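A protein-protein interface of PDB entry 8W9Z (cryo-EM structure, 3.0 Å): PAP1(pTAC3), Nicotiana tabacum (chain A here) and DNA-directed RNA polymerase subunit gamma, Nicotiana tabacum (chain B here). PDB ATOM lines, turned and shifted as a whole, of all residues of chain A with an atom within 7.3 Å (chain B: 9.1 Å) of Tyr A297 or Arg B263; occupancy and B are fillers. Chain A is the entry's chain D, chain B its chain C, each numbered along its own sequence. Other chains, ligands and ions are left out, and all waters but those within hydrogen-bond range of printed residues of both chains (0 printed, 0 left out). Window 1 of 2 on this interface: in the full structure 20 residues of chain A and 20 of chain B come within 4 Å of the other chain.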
ATOM      1  N   TYR A 291     -34.444 -11.585  11.799  1.00  0.00           N
ATOM      2  CA  TYR A 291     -33.492 -10.839  10.982  1.00  0.00           C
ATOM      3  C   TYR A 291     -32.041 -11.136  11.334  1.00  0.00           C
ATOM      4  O   TYR A 291     -31.148 -10.804  10.547  1.00  0.00           O
ATOM      5  CB  TYR A 291     -33.747  -9.336  11.104  1.00  0.00           C
ATOM      6  CG  TYR A 291     -34.698  -8.797  10.063  1.00  0.00           C
ATOM      7  CD1 TYR A 291     -34.286  -8.620   8.751  1.00  0.00           C
ATOM      8  CD2 TYR A 291     -36.004  -8.464  10.388  1.00  0.00           C
ATOM      9  CE1 TYR A 291     -35.146  -8.131   7.791  1.00  0.00           C
ATOM     10  CE2 TYR A 291     -36.873  -7.972   9.434  1.00  0.00           C
ATOM     11  CZ  TYR A 291     -36.437  -7.807   8.137  1.00  0.00           C
ATOM     12  OH  TYR A 291     -37.294  -7.318   7.179  1.00  0.00           O
ATOM     13  N   THR A 292     -31.782 -11.748  12.490  1.00  0.00           N
ATOM     14  CA  THR A 292     -30.408 -12.013  12.907  1.00  0.00           C
ATOM     15  C   THR A 292     -29.923 -13.370  12.410  1.00  0.00           C
ATOM     16  O   THR A 292     -28.817 -13.485  11.870  1.00  0.00           O
ATOM     17  CB  THR A 292     -30.300 -11.936  14.432  1.00  0.00           C
ATOM     18  OG1 THR A 292     -30.572 -10.598  14.865  1.00  0.00           O
ATOM     19  CG2 THR A 292     -28.911 -12.342  14.894  1.00  0.00           C
ATOM     20  N   ARG A 293     -30.743 -14.409  12.575  1.00  0.00           N
ATOM     21  CA  ARG A 293     -30.362 -15.775  12.238  1.00  0.00           C
ATOM     22  C   ARG A 293     -30.705 -16.149  10.800  1.00  0.00           C
ATOM     23  O   ARG A 293     -30.905 -17.334  10.503  1.00  0.00           O
ATOM     24  CB  ARG A 293     -31.014 -16.753  13.214  1.00  0.00           C
ATOM     25  CG  ARG A 293     -30.582 -16.554  14.657  1.00  0.00           C
ATOM     26  CD  ARG A 293     -31.346 -17.466  15.600  1.00  0.00           C
ATOM     27  NE  ARG A 293     -30.946 -17.265  16.989  1.00  0.00           N
ATOM     28  CZ  ARG A 293     -31.489 -17.900  18.022  1.00  0.00           C
ATOM     29  NH1 ARG A 293     -32.460 -18.780  17.825  1.00  0.00           N
ATOM     30  NH2 ARG A 293     -31.063 -17.654  19.252  1.00  0.00           N
ATOM     31  N   ALA A 294     -30.778 -15.174   9.900  1.00  0.00           N
ATOM     32  CA  ALA A 294     -31.037 -15.462   8.501  1.00  0.00           C
ATOM     33  C   ALA A 294     -29.763 -15.938   7.810  1.00  0.00           C
ATOM     34  O   ALA A 294     -28.650 -15.783   8.322  1.00  0.00           O
ATOM     35  CB  ALA A 294     -31.594 -14.230   7.790  1.00  0.00           C
ATOM     36  N   GLU A 295     -29.939 -16.527   6.627  1.00  0.00           N
ATOM     37  CA  GLU A 295     -28.830 -17.073   5.855  1.00  0.00           C
ATOM     38  C   GLU A 295     -28.933 -16.682   4.385  1.00  0.00           C
ATOM     39  O   GLU A 295     -28.599 -17.475   3.502  1.00  0.00           O
ATOM     40  CB  GLU A 295     -28.766 -18.595   5.995  1.00  0.00           C
ATOM     41  CG  GLU A 295     -28.551 -19.086   7.418  1.00  0.00           C
ATOM     42  CD  GLU A 295     -28.602 -20.597   7.528  1.00  0.00           C
ATOM     43  OE1 GLU A 295     -28.780 -21.264   6.487  1.00  0.00           O
ATOM     44  OE2 GLU A 295     -28.465 -21.118   8.655  1.00  0.00           O
ATOM     45  N   SER A 296     -29.392 -15.464   4.105  1.00  0.00           N
ATOM     46  CA  SER A 296     -29.610 -15.027   2.732  1.00  0.00           C
ATOM     47  C   SER A 296     -28.744 -13.843   2.337  1.00  0.00           C
ATOM     48  O   SER A 296     -28.018 -13.921   1.340  1.00  0.00           O
ATOM     49  CB  SER A 296     -31.094 -14.684   2.524  1.00  0.00           C
ATOM     50  OG  SER A 296     -31.918 -15.803   2.796  1.00  0.00           O
ATOM     51  N   TYR A 297     -28.791 -12.746   3.090  1.00  0.00           N
ATOM     52  CA  TYR A 297     -28.093 -11.525   2.706  1.00  0.00           C
ATOM     53  C   TYR A 297     -27.586 -10.834   3.967  1.00  0.00           C
ATOM     54  O   TYR A 297     -27.479 -11.449   5.032  1.00  0.00           O
ATOM     55  CB  TYR A 297     -29.006 -10.619   1.870  1.00  0.00           C
ATOM     56  CG  TYR A 297     -29.400 -11.222   0.542  1.00  0.00           C
ATOM     57  CD1 TYR A 297     -28.558 -11.138  -0.558  1.00  0.00           C
ATOM     58  CD2 TYR A 297     -30.612 -11.879   0.389  1.00  0.00           C
ATOM     59  CE1 TYR A 297     -28.914 -11.692  -1.773  1.00  0.00           C
ATOM     60  CE2 TYR A 297     -30.975 -12.435  -0.819  1.00  0.00           C
ATOM     61  CZ  TYR A 297     -30.124 -12.338  -1.897  1.00  0.00           C
ATOM     62  OH  TYR A 297     -30.486 -12.891  -3.102  1.00  0.00           O
ATOM     63  N   ASP A 298     -27.257  -9.545   3.835  1.00  0.00           N
ATOM     64  CA  ASP A 298     -26.596  -8.820   4.916  1.00  0.00           C
ATOM     65  C   ASP A 298     -27.479  -8.740   6.157  1.00  0.00           C
ATOM     66  O   ASP A 298     -27.170  -9.335   7.194  1.00  0.00           O
ATOM     67  CB  ASP A 298     -26.209  -7.420   4.434  1.00  0.00           C
ATOM     68  CG  ASP A 298     -25.188  -6.753   5.334  1.00  0.00           C
ATOM     69  OD1 ASP A 298     -24.751  -7.388   6.317  1.00  0.00           O
ATOM     70  OD2 ASP A 298     -24.818  -5.594   5.057  1.00  0.00           O
ATOM     71  N   ARG A 299     -28.596  -8.012   6.060  1.00  0.00           N
ATOM     72  CA  ARG A 299     -29.551  -7.866   7.162  1.00  0.00           C
ATOM     73  C   ARG A 299     -28.881  -7.302   8.416  1.00  0.00           C
ATOM     74  O   ARG A 299     -28.973  -7.869   9.506  1.00  0.00           O
ATOM     75  CB  ARG A 299     -30.251  -9.194   7.468  1.00  0.00           C
ATOM     76  CG  ARG A 299     -31.439  -9.516   6.572  1.00  0.00           C
ATOM     77  CD  ARG A 299     -31.009  -9.888   5.167  1.00  0.00           C
ATOM     78  NE  ARG A 299     -32.150 -10.193   4.311  1.00  0.00           N
ATOM     79  CZ  ARG A 299     -32.683 -11.403   4.184  1.00  0.00           C
ATOM     80  NH1 ARG A 299     -32.175 -12.424   4.859  1.00  0.00           N
ATOM     81  NH2 ARG A 299     -33.721 -11.592   3.383  1.00  0.00           N
ATOM     82  N   VAL A 300     -28.202  -6.167   8.256  1.00  0.00           N
ATOM     83  CA  VAL A 300     -27.556  -5.502   9.383  1.00  0.00           C
ATOM     84  C   VAL A 300     -28.149  -4.109   9.550  1.00  0.00           C
ATOM     85  O   VAL A 300     -28.150  -3.550  10.652  1.00  0.00           O
ATOM     86  CB  VAL A 300     -26.026  -5.443   9.202  1.00  0.00           C
ATOM     87  CG1 VAL A 300     -25.649  -4.535   8.040  1.00  0.00           C
ATOM     88  CG2 VAL A 300     -25.353  -4.989  10.490  1.00  0.00           C
ATOM     89  N   LYS A 333     -21.789 -10.750  15.570  1.00  0.00           N
ATOM     90  CA  LYS A 333     -21.657 -11.522  14.338  1.00  0.00           C
ATOM     91  C   LYS A 333     -21.382 -10.655  13.117  1.00  0.00           C
ATOM     92  O   LYS A 333     -21.029 -11.198  12.064  1.00  0.00           O
ATOM     93  CB  LYS A 333     -22.917 -12.359  14.104  1.00  0.00           C
ATOM     94  CG  LYS A 333     -23.084 -13.514  15.076  1.00  0.00           C
ATOM     95  CD  LYS A 333     -24.375 -14.274  14.818  1.00  0.00           C
ATOM     96  CE  LYS A 333     -24.408 -14.843  13.411  1.00  0.00           C
ATOM     97  NZ  LYS A 333     -23.279 -15.781  13.165  1.00  0.00           N
ATOM     98  N   TYR A 334     -21.533  -9.334  13.221  1.00  0.00           N
ATOM     99  CA  TYR A 334     -21.263  -8.424  12.116  1.00  0.00           C
ATOM    100  C   TYR A 334     -20.071  -7.513  12.392  1.00  0.00           C
ATOM    101  O   TYR A 334     -19.954  -6.449  11.775  1.00  0.00           O
ATOM    102  CB  TYR A 334     -22.505  -7.594  11.795  1.00  0.00           C
ATOM    103  CG  TYR A 334     -23.586  -8.369  11.077  1.00  0.00           C
ATOM    104  CD1 TYR A 334     -24.476  -9.169  11.778  1.00  0.00           C
ATOM    105  CD2 TYR A 334     -23.717  -8.299   9.698  1.00  0.00           C
ATOM    106  CE1 TYR A 334     -25.464  -9.879  11.126  1.00  0.00           C
ATOM    107  CE2 TYR A 334     -24.701  -9.005   9.040  1.00  0.00           C
ATOM    108  CZ  TYR A 334     -25.571  -9.793   9.758  1.00  0.00           C
ATOM    109  OH  TYR A 334     -26.554 -10.499   9.103  1.00  0.00           O
ATOM    110  N   LYS A 454     -15.436 -20.798  -1.452  1.00  0.00           N
ATOM    111  CA  LYS A 454     -15.585 -19.690  -0.507  1.00  0.00           C
ATOM    112  C   LYS A 454     -16.034 -20.235   0.850  1.00  0.00           C
ATOM    113  O   LYS A 454     -17.170 -20.063   1.296  1.00  0.00           O
ATOM    114  CB  LYS A 454     -16.555 -18.650  -1.053  1.00  0.00           C
ATOM    115  CG  LYS A 454     -17.801 -19.227  -1.701  1.00  0.00           C
ATOM    116  CD  LYS A 454     -18.639 -18.131  -2.335  1.00  0.00           C
ATOM    117  CE  LYS A 454     -19.843 -18.702  -3.063  1.00  0.00           C
ATOM    118  NZ  LYS A 454     -20.611 -17.636  -3.762  1.00  0.00           N
ATOM    119  N   PHE A 464     -18.650 -16.115  12.582  1.00  0.00           N
ATOM    120  CA  PHE A 464     -18.739 -14.764  12.048  1.00  0.00           C
ATOM    121  C   PHE A 464     -19.244 -14.785  10.609  1.00  0.00           C
ATOM    122  O   PHE A 464     -18.983 -15.718   9.846  1.00  0.00           O
ATOM    123  CB  PHE A 464     -17.382 -14.069  12.127  1.00  0.00           C
ATOM    124  CG  PHE A 464     -16.957 -13.735  13.527  1.00  0.00           C
ATOM    125  CD1 PHE A 464     -16.375 -14.694  14.336  1.00  0.00           C
ATOM    126  CD2 PHE A 464     -17.145 -12.463  14.037  1.00  0.00           C
ATOM    127  CE1 PHE A 464     -15.986 -14.392  15.623  1.00  0.00           C
ATOM    128  CE2 PHE A 464     -16.758 -12.154  15.324  1.00  0.00           C
ATOM    129  CZ  PHE A 464     -16.177 -13.120  16.118  1.00  0.00           C
ATOM    130  N   ILE A 465     -19.981 -13.735  10.247  1.00  0.00           N
ATOM    131  CA  ILE A 465     -20.617 -13.683   8.933  1.00  0.00           C
ATOM    132  C   ILE A 465     -19.570 -13.524   7.837  1.00  0.00           C
ATOM    133  O   ILE A 465     -19.461 -14.359   6.932  1.00  0.00           O
ATOM    134  CB  ILE A 465     -21.659 -12.553   8.883  1.00  0.00           C
ATOM    135  CG1 ILE A 465     -22.801 -12.837   9.860  1.00  0.00           C
ATOM    136  CG2 ILE A 465     -22.194 -12.385   7.474  1.00  0.00           C
ATOM    137  CD1 ILE A 465     -23.547 -14.121   9.569  1.00  0.00           C
ATOM    138  N   TYR A 466     -18.784 -12.450   7.902  1.00  0.00           N
ATOM    139  CA  TYR A 466     -17.797 -12.173   6.864  1.00  0.00           C
ATOM    140  C   TYR A 466     -16.433 -12.768   7.207  1.00  0.00           C
ATOM    141  O   TYR A 466     -15.923 -13.624   6.478  1.00  0.00           O
ATOM    142  CB  TYR A 466     -17.684 -10.662   6.641  1.00  0.00           C
ATOM    143  CG  TYR A 466     -18.908 -10.045   6.007  1.00  0.00           C
ATOM    144  CD1 TYR A 466     -19.804 -10.821   5.285  1.00  0.00           C
ATOM    145  CD2 TYR A 466     -19.166  -8.688   6.124  1.00  0.00           C
ATOM    146  CE1 TYR A 466     -20.924 -10.263   4.702  1.00  0.00           C
ATOM    147  CE2 TYR A 466     -20.282  -8.121   5.545  1.00  0.00           C
ATOM    148  CZ  TYR A 466     -21.157  -8.912   4.834  1.00  0.00           C
ATOM    149  OH  TYR A 466     -22.272  -8.352   4.256  1.00  0.00           O
ATOM    150  N   GLN B  16     -41.326 -13.981  -4.719  1.00  0.00           N
ATOM    151  CA  GLN B  16     -39.967 -13.450  -4.776  1.00  0.00           C
ATOM    152  C   GLN B  16     -39.326 -13.833  -6.103  1.00  0.00           C
ATOM    153  O   GLN B  16     -38.940 -14.989  -6.301  1.00  0.00           O
ATOM    154  CB  GLN B  16     -39.131 -13.951  -3.597  1.00  0.00           C
ATOM    155  CG  GLN B  16     -39.283 -15.427  -3.281  1.00  0.00           C
ATOM    156  CD  GLN B  16     -38.236 -15.918  -2.303  1.00  0.00           C
ATOM    157  OE1 GLN B  16     -37.384 -15.152  -1.854  1.00  0.00           O
ATOM    158  NE2 GLN B  16     -38.293 -17.201  -1.969  1.00  0.00           N
ATOM    159  N   LEU B  17     -39.201 -12.864  -7.003  1.00  0.00           N
ATOM    160  CA  LEU B  17     -38.540 -13.078  -8.285  1.00  0.00           C
ATOM    161  C   LEU B  17     -37.051 -12.797  -8.124  1.00  0.00           C
ATOM    162  O   LEU B  17     -36.657 -11.665  -7.819  1.00  0.00           O
ATOM    163  CB  LEU B  17     -39.154 -12.188  -9.365  1.00  0.00           C
ATOM    164  CG  LEU B  17     -38.817 -12.532 -10.816  1.00  0.00           C
ATOM    165  CD1 LEU B  17     -40.022 -12.294 -11.709  1.00  0.00           C
ATOM    166  CD2 LEU B  17     -37.624 -11.726 -11.305  1.00  0.00           C
ATOM    167  N   ARG B  18     -36.229 -13.822  -8.331  1.00  0.00           N
ATOM    168  CA  ARG B  18     -34.795 -13.743  -8.101  1.00  0.00           C
ATOM    169  C   ARG B  18     -34.044 -13.782  -9.426  1.00  0.00           C
ATOM    170  O   ARG B  18     -34.401 -14.540 -10.332  1.00  0.00           O
ATOM    171  CB  ARG B  18     -34.324 -14.889  -7.201  1.00  0.00           C
ATOM    172  CG  ARG B  18     -32.841 -14.862  -6.887  1.00  0.00           C
ATOM    173  CD  ARG B  18     -32.419 -16.085  -6.093  1.00  0.00           C
ATOM    174  NE  ARG B  18     -30.970 -16.151  -5.937  1.00  0.00           N
ATOM    175  CZ  ARG B  18     -30.151 -16.711  -6.820  1.00  0.00           C
ATOM    176  NH1 ARG B  18     -30.639 -17.258  -7.925  1.00  0.00           N
ATOM    177  NH2 ARG B  18     -28.844 -16.726  -6.600  1.00  0.00           N
ATOM    178  N   ILE B  19     -33.001 -12.960  -9.531  1.00  0.00           N
ATOM    179  CA  ILE B  19     -32.162 -12.894 -10.718  1.00  0.00           C
ATOM    180  C   ILE B  19     -30.731 -13.228 -10.319  1.00  0.00           C
ATOM    181  O   ILE B  19     -30.305 -12.972  -9.188  1.00  0.00           O
ATOM    182  CB  ILE B  19     -32.240 -11.509 -11.401  1.00  0.00           C
ATOM    183  CG1 ILE B  19     -31.607 -11.551 -12.793  1.00  0.00           C
ATOM    184  CG2 ILE B  19     -31.575 -10.442 -10.541  1.00  0.00           C
ATOM    185  CD1 ILE B  19     -31.669 -10.232 -13.532  1.00  0.00           C
ATOM    186  N   GLY B  20     -29.994 -13.822 -11.251  1.00  0.00           N
ATOM    187  CA  GLY B  20     -28.609 -14.173 -10.994  1.00  0.00           C
ATOM    188  C   GLY B  20     -27.918 -14.594 -12.270  1.00  0.00           C
ATOM    189  O   GLY B  20     -28.552 -14.820 -13.305  1.00  0.00           O
ATOM    190  N   LEU B 215     -11.773 -13.852  -1.028  1.00  0.00           N
ATOM    191  CA  LEU B 215     -12.665 -12.716  -0.839  1.00  0.00           C
ATOM    192  C   LEU B 215     -12.730 -12.232   0.603  1.00  0.00           C
ATOM    193  O   LEU B 215     -13.438 -11.256   0.877  1.00  0.00           O
ATOM    194  CB  LEU B 215     -14.071 -13.073  -1.324  1.00  0.00           C
ATOM    195  CG  LEU B 215     -14.190 -13.391  -2.814  1.00  0.00           C
ATOM    196  CD1 LEU B 215     -15.564 -13.947  -3.136  1.00  0.00           C
ATOM    197  CD2 LEU B 215     -13.903 -12.151  -3.645  1.00  0.00           C
ATOM    198  N   ARG B 216     -12.020 -12.874   1.529  1.00  0.00           N
ATOM    199  CA  ARG B 216     -12.017 -12.443   2.921  1.00  0.00           C
ATOM    200  C   ARG B 216     -10.783 -11.640   3.300  1.00  0.00           C
ATOM    201  O   ARG B 216     -10.847 -10.834   4.233  1.00  0.00           O
ATOM    202  CB  ARG B 216     -12.145 -13.653   3.853  1.00  0.00           C
ATOM    203  CG  ARG B 216     -13.499 -14.338   3.775  1.00  0.00           C
ATOM    204  CD  ARG B 216     -13.651 -15.404   4.843  1.00  0.00           C
ATOM    205  NE  ARG B 216     -14.994 -15.975   4.847  1.00  0.00           N
ATOM    206  CZ  ARG B 216     -15.356 -17.040   4.139  1.00  0.00           C
ATOM    207  NH1 ARG B 216     -14.472 -17.658   3.368  1.00  0.00           N
ATOM    208  NH2 ARG B 216     -16.602 -17.489   4.204  1.00  0.00           N
ATOM    209  N   LEU B 257     -18.512  -4.527  -3.452  1.00  0.00           N
ATOM    210  CA  LEU B 257     -18.654  -5.641  -4.384  1.00  0.00           C
ATOM    211  C   LEU B 257     -18.162  -6.942  -3.761  1.00  0.00           C
ATOM    212  O   LEU B 257     -18.744  -8.007  -3.994  1.00  0.00           O
ATOM    213  CB  LEU B 257     -17.894  -5.336  -5.675  1.00  0.00           C
ATOM    214  CG  LEU B 257     -18.506  -5.764  -7.011  1.00  0.00           C
ATOM    215  CD1 LEU B 257     -17.704  -5.182  -8.163  1.00  0.00           C
ATOM    216  CD2 LEU B 257     -18.586  -7.276  -7.133  1.00  0.00           C
ATOM    217  N   ALA B 258     -17.096  -6.876  -2.964  1.00  0.00           N
ATOM    218  CA  ALA B 258     -16.536  -8.082  -2.371  1.00  0.00           C
ATOM    219  C   ALA B 258     -17.376  -8.604  -1.213  1.00  0.00           C
ATOM    220  O   ALA B 258     -17.403  -9.816  -0.976  1.00  0.00           O
ATOM    221  CB  ALA B 258     -15.104  -7.822  -1.902  1.00  0.00           C
ATOM    222  N   LYS B 259     -18.063  -7.720  -0.483  1.00  0.00           N
ATOM    223  CA  LYS B 259     -18.887  -8.188   0.629  1.00  0.00           C
ATOM    224  C   LYS B 259     -20.097  -8.979   0.148  1.00  0.00           C
ATOM    225  O   LYS B 259     -20.605  -9.834   0.882  1.00  0.00           O
ATOM    226  CB  LYS B 259     -19.338  -7.012   1.494  1.00  0.00           C
ATOM    227  CG  LYS B 259     -18.235  -6.402   2.343  1.00  0.00           C
ATOM    228  CD  LYS B 259     -18.810  -5.529   3.447  1.00  0.00           C
ATOM    229  CE  LYS B 259     -19.721  -4.450   2.886  1.00  0.00           C
ATOM    230  NZ  LYS B 259     -18.999  -3.536   1.960  1.00  0.00           N
ATOM    231  N   HIS B 260     -20.572  -8.714  -1.071  1.00  0.00           N
ATOM    232  CA  HIS B 260     -21.752  -9.414  -1.570  1.00  0.00           C
ATOM    233  C   HIS B 260     -21.444 -10.869  -1.902  1.00  0.00           C
ATOM    234  O   HIS B 260     -22.209 -11.768  -1.537  1.00  0.00           O
ATOM    235  CB  HIS B 260     -22.315  -8.694  -2.794  1.00  0.00           C
ATOM    236  CG  HIS B 260     -23.234  -7.562  -2.459  1.00  0.00           C
ATOM    237  ND1 HIS B 260     -24.596  -7.624  -2.664  1.00  0.00           N
ATOM    238  CD2 HIS B 260     -22.990  -6.342  -1.926  1.00  0.00           C
ATOM    239  CE1 HIS B 260     -25.149  -6.490  -2.276  1.00  0.00           C
ATOM    240  NE2 HIS B 260     -24.198  -5.695  -1.824  1.00  0.00           N
ATOM    241  N   PHE B 261     -20.325 -11.121  -2.587  1.00  0.00           N
ATOM    242  CA  PHE B 261     -20.009 -12.472  -3.041  1.00  0.00           C
ATOM    243  C   PHE B 261     -19.803 -13.449  -1.893  1.00  0.00           C
ATOM    244  O   PHE B 261     -19.834 -14.664  -2.117  1.00  0.00           O
ATOM    245  CB  PHE B 261     -18.766 -12.448  -3.928  1.00  0.00           C
ATOM    246  CG  PHE B 261     -19.028 -11.972  -5.325  1.00  0.00           C
ATOM    247  CD1 PHE B 261     -20.239 -12.227  -5.943  1.00  0.00           C
ATOM    248  CD2 PHE B 261     -18.063 -11.270  -6.023  1.00  0.00           C
ATOM    249  CE1 PHE B 261     -20.482 -11.791  -7.228  1.00  0.00           C
ATOM    250  CE2 PHE B 261     -18.300 -10.831  -7.307  1.00  0.00           C
ATOM    251  CZ  PHE B 261     -19.511 -11.092  -7.911  1.00  0.00           C
ATOM    252  N   ILE B 262     -19.590 -12.955  -0.672  1.00  0.00           N
ATOM    253  CA  ILE B 262     -19.376 -13.855   0.453  1.00  0.00           C
ATOM    254  C   ILE B 262     -20.685 -14.497   0.892  1.00  0.00           C
ATOM    255  O   ILE B 262     -20.689 -15.607   1.435  1.00  0.00           O
ATOM    256  CB  ILE B 262     -18.700 -13.100   1.613  1.00  0.00           C
ATOM    257  CG1 ILE B 262     -17.519 -12.280   1.094  1.00  0.00           C
ATOM    258  CG2 ILE B 262     -18.231 -14.070   2.683  1.00  0.00           C
ATOM    259  CD1 ILE B 262     -16.807 -11.489   2.168  1.00  0.00           C
ATOM    260  N   ARG B 263     -21.813 -13.829   0.655  1.00  0.00           N
ATOM    261  CA  ARG B 263     -23.100 -14.281   1.171  1.00  0.00           C
ATOM    262  C   ARG B 263     -24.176 -14.189   0.096  1.00  0.00           C
ATOM    263  O   ARG B 263     -25.299 -13.747   0.356  1.00  0.00           O
ATOM    264  CB  ARG B 263     -23.501 -13.473   2.404  1.00  0.00           C
ATOM    265  CG  ARG B 263     -24.183 -14.277   3.496  1.00  0.00           C
ATOM    266  CD  ARG B 263     -24.364 -13.431   4.745  1.00  0.00           C
ATOM    267  NE  ARG B 263     -24.865 -14.206   5.875  1.00  0.00           N
ATOM    268  CZ  ARG B 263     -26.149 -14.304   6.202  1.00  0.00           C
ATOM    269  NH1 ARG B 263     -27.067 -13.675   5.483  1.00  0.00           N
ATOM    270  NH2 ARG B 263     -26.514 -15.031   7.249  1.00  0.00           N
ATOM    271  N   THR B 264     -23.850 -14.606  -1.130  1.00  0.00           N
ATOM    272  CA  THR B 264     -24.823 -14.576  -2.213  1.00  0.00           C
ATOM    273  C   THR B 264     -24.821 -15.827  -3.081  1.00  0.00           C
ATOM    274  O   THR B 264     -25.588 -15.876  -4.047  1.00  0.00           O
ATOM    275  CB  THR B 264     -24.595 -13.349  -3.111  1.00  0.00           C
ATOM    276  OG1 THR B 264     -25.731 -13.165  -3.967  1.00  0.00           O
ATOM    277  CG2 THR B 264     -23.357 -13.542  -3.970  1.00  0.00           C
ATOM    278  N   ASN B 265     -23.971 -16.815  -2.792  1.00  0.00           N
ATOM    279  CA  ASN B 265     -23.915 -18.099  -3.491  1.00  0.00           C
ATOM    280  C   ASN B 265     -23.563 -17.949  -4.969  1.00  0.00           C
ATOM    281  O   ASN B 265     -23.533 -18.940  -5.706  1.00  0.00           O
ATOM    282  CB  ASN B 265     -25.237 -18.866  -3.319  1.00  0.00           C
ATOM    283  N   ILE B 266     -23.261 -16.731  -5.407  1.00  0.00           N
ATOM    284  CA  ILE B 266     -22.865 -16.462  -6.785  1.00  0.00           C
ATOM    285  C   ILE B 266     -21.346 -16.366  -6.833  1.00  0.00           C
ATOM    286  O   ILE B 266     -20.751 -15.481  -6.208  1.00  0.00           O
ATOM    287  CB  ILE B 266     -23.518 -15.178  -7.320  1.00  0.00           C
ATOM    288  CG1 ILE B 266     -25.032 -15.357  -7.430  1.00  0.00           C
ATOM    289  CG2 ILE B 266     -22.927 -14.799  -8.668  1.00  0.00           C
ATOM    290  CD1 ILE B 266     -25.446 -16.474  -8.361  1.00  0.00           C
ATOM    291  N   GLU B 267     -20.718 -17.277  -7.577  1.00  0.00           N
ATOM    292  CA  GLU B 267     -19.265 -17.302  -7.686  1.00  0.00           C
ATOM    293  C   GLU B 267     -18.795 -16.271  -8.711  1.00  0.00           C
ATOM    294  O   GLU B 267     -19.465 -16.048  -9.721  1.00  0.00           O
ATOM    295  CB  GLU B 267     -18.784 -18.694  -8.087  1.00  0.00           C
ATOM    296  CG  GLU B 267     -19.107 -19.773  -7.067  1.00  0.00           C
ATOM    297  CD  GLU B 267     -18.715 -21.159  -7.538  1.00  0.00           C
ATOM    298  OE1 GLU B 267     -18.378 -21.310  -8.731  1.00  0.00           O
ATOM    299  OE2 GLU B 267     -18.743 -22.098  -6.715  1.00  0.00           O
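O of Tyr A466 is in hydrogen-bond range of NE of Arg B216. The backbone carbonyl oxygen of Phe B261 sits at hydrogen-bond distance from the side-chain amino group of Lys A454 (3.5 Å). The backbone carbonyl oxygen (O) of Ala A294 sits at hydrogen-bond distance from the guanidinium group (NH2) of Arg B263 (2.5 Å). NZ of Lys A454 sits at hydrogen-bond distance from O of Ile B266 (3.3 Å). The backbone carbonyl oxygen of Ser A296 lies close to the backbone carbonyl oxygen of Arg B263, 2.9 Å away. The backbone carbonyl oxygen of Tyr A297 sits close to the guanidinium group of Arg B263, at 2.3 Å.
The side-chain hydroxyl of Tyr A466 sits at hydrogen-bond distance from the side-chain carboxylate of Asp A298, 3.4 Å away. O of Lys A333 sits close to N of Ile A465, 3.3 Å away.
Among the printed residues, pairs that only touch across the chains: Glu A295 with Arg B263 (3.4 Å), Lys A454 with Arg B216 (3.9 Å), Lys A454 with Asn B265 (3.2 Å), Lys A454 with Glu B267 (3.8 Å), Ile A465 with Arg B263 (3.6 Å) and Tyr A466 with Lys B259 (3.6 Å).
Tyr A297 touches just one residue of chain B: Arg B263. Of the printed residues of chain B, Tyr A466 touches Arg B216 and Lys B259. Thr B264 touches none of the printed residues of chain A. Printed residues of chain A within 4 Å of Ile B266: Lys A454 (3.2 Å). The nearest printed residue of chain A that does not touch Asn B265 is Ser A296 (6.5 Å).
Of the 16 printed residues of chain A, 7 touch a printed residue of chain B. Printed residues of chain A that touch a printed residue of chain B: Ala A294, Glu A295, Ser A296, Tyr A297, Lys A454, Ile A465 and Tyr A466. Among the printed residues, 12 pairs touch across the chains.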
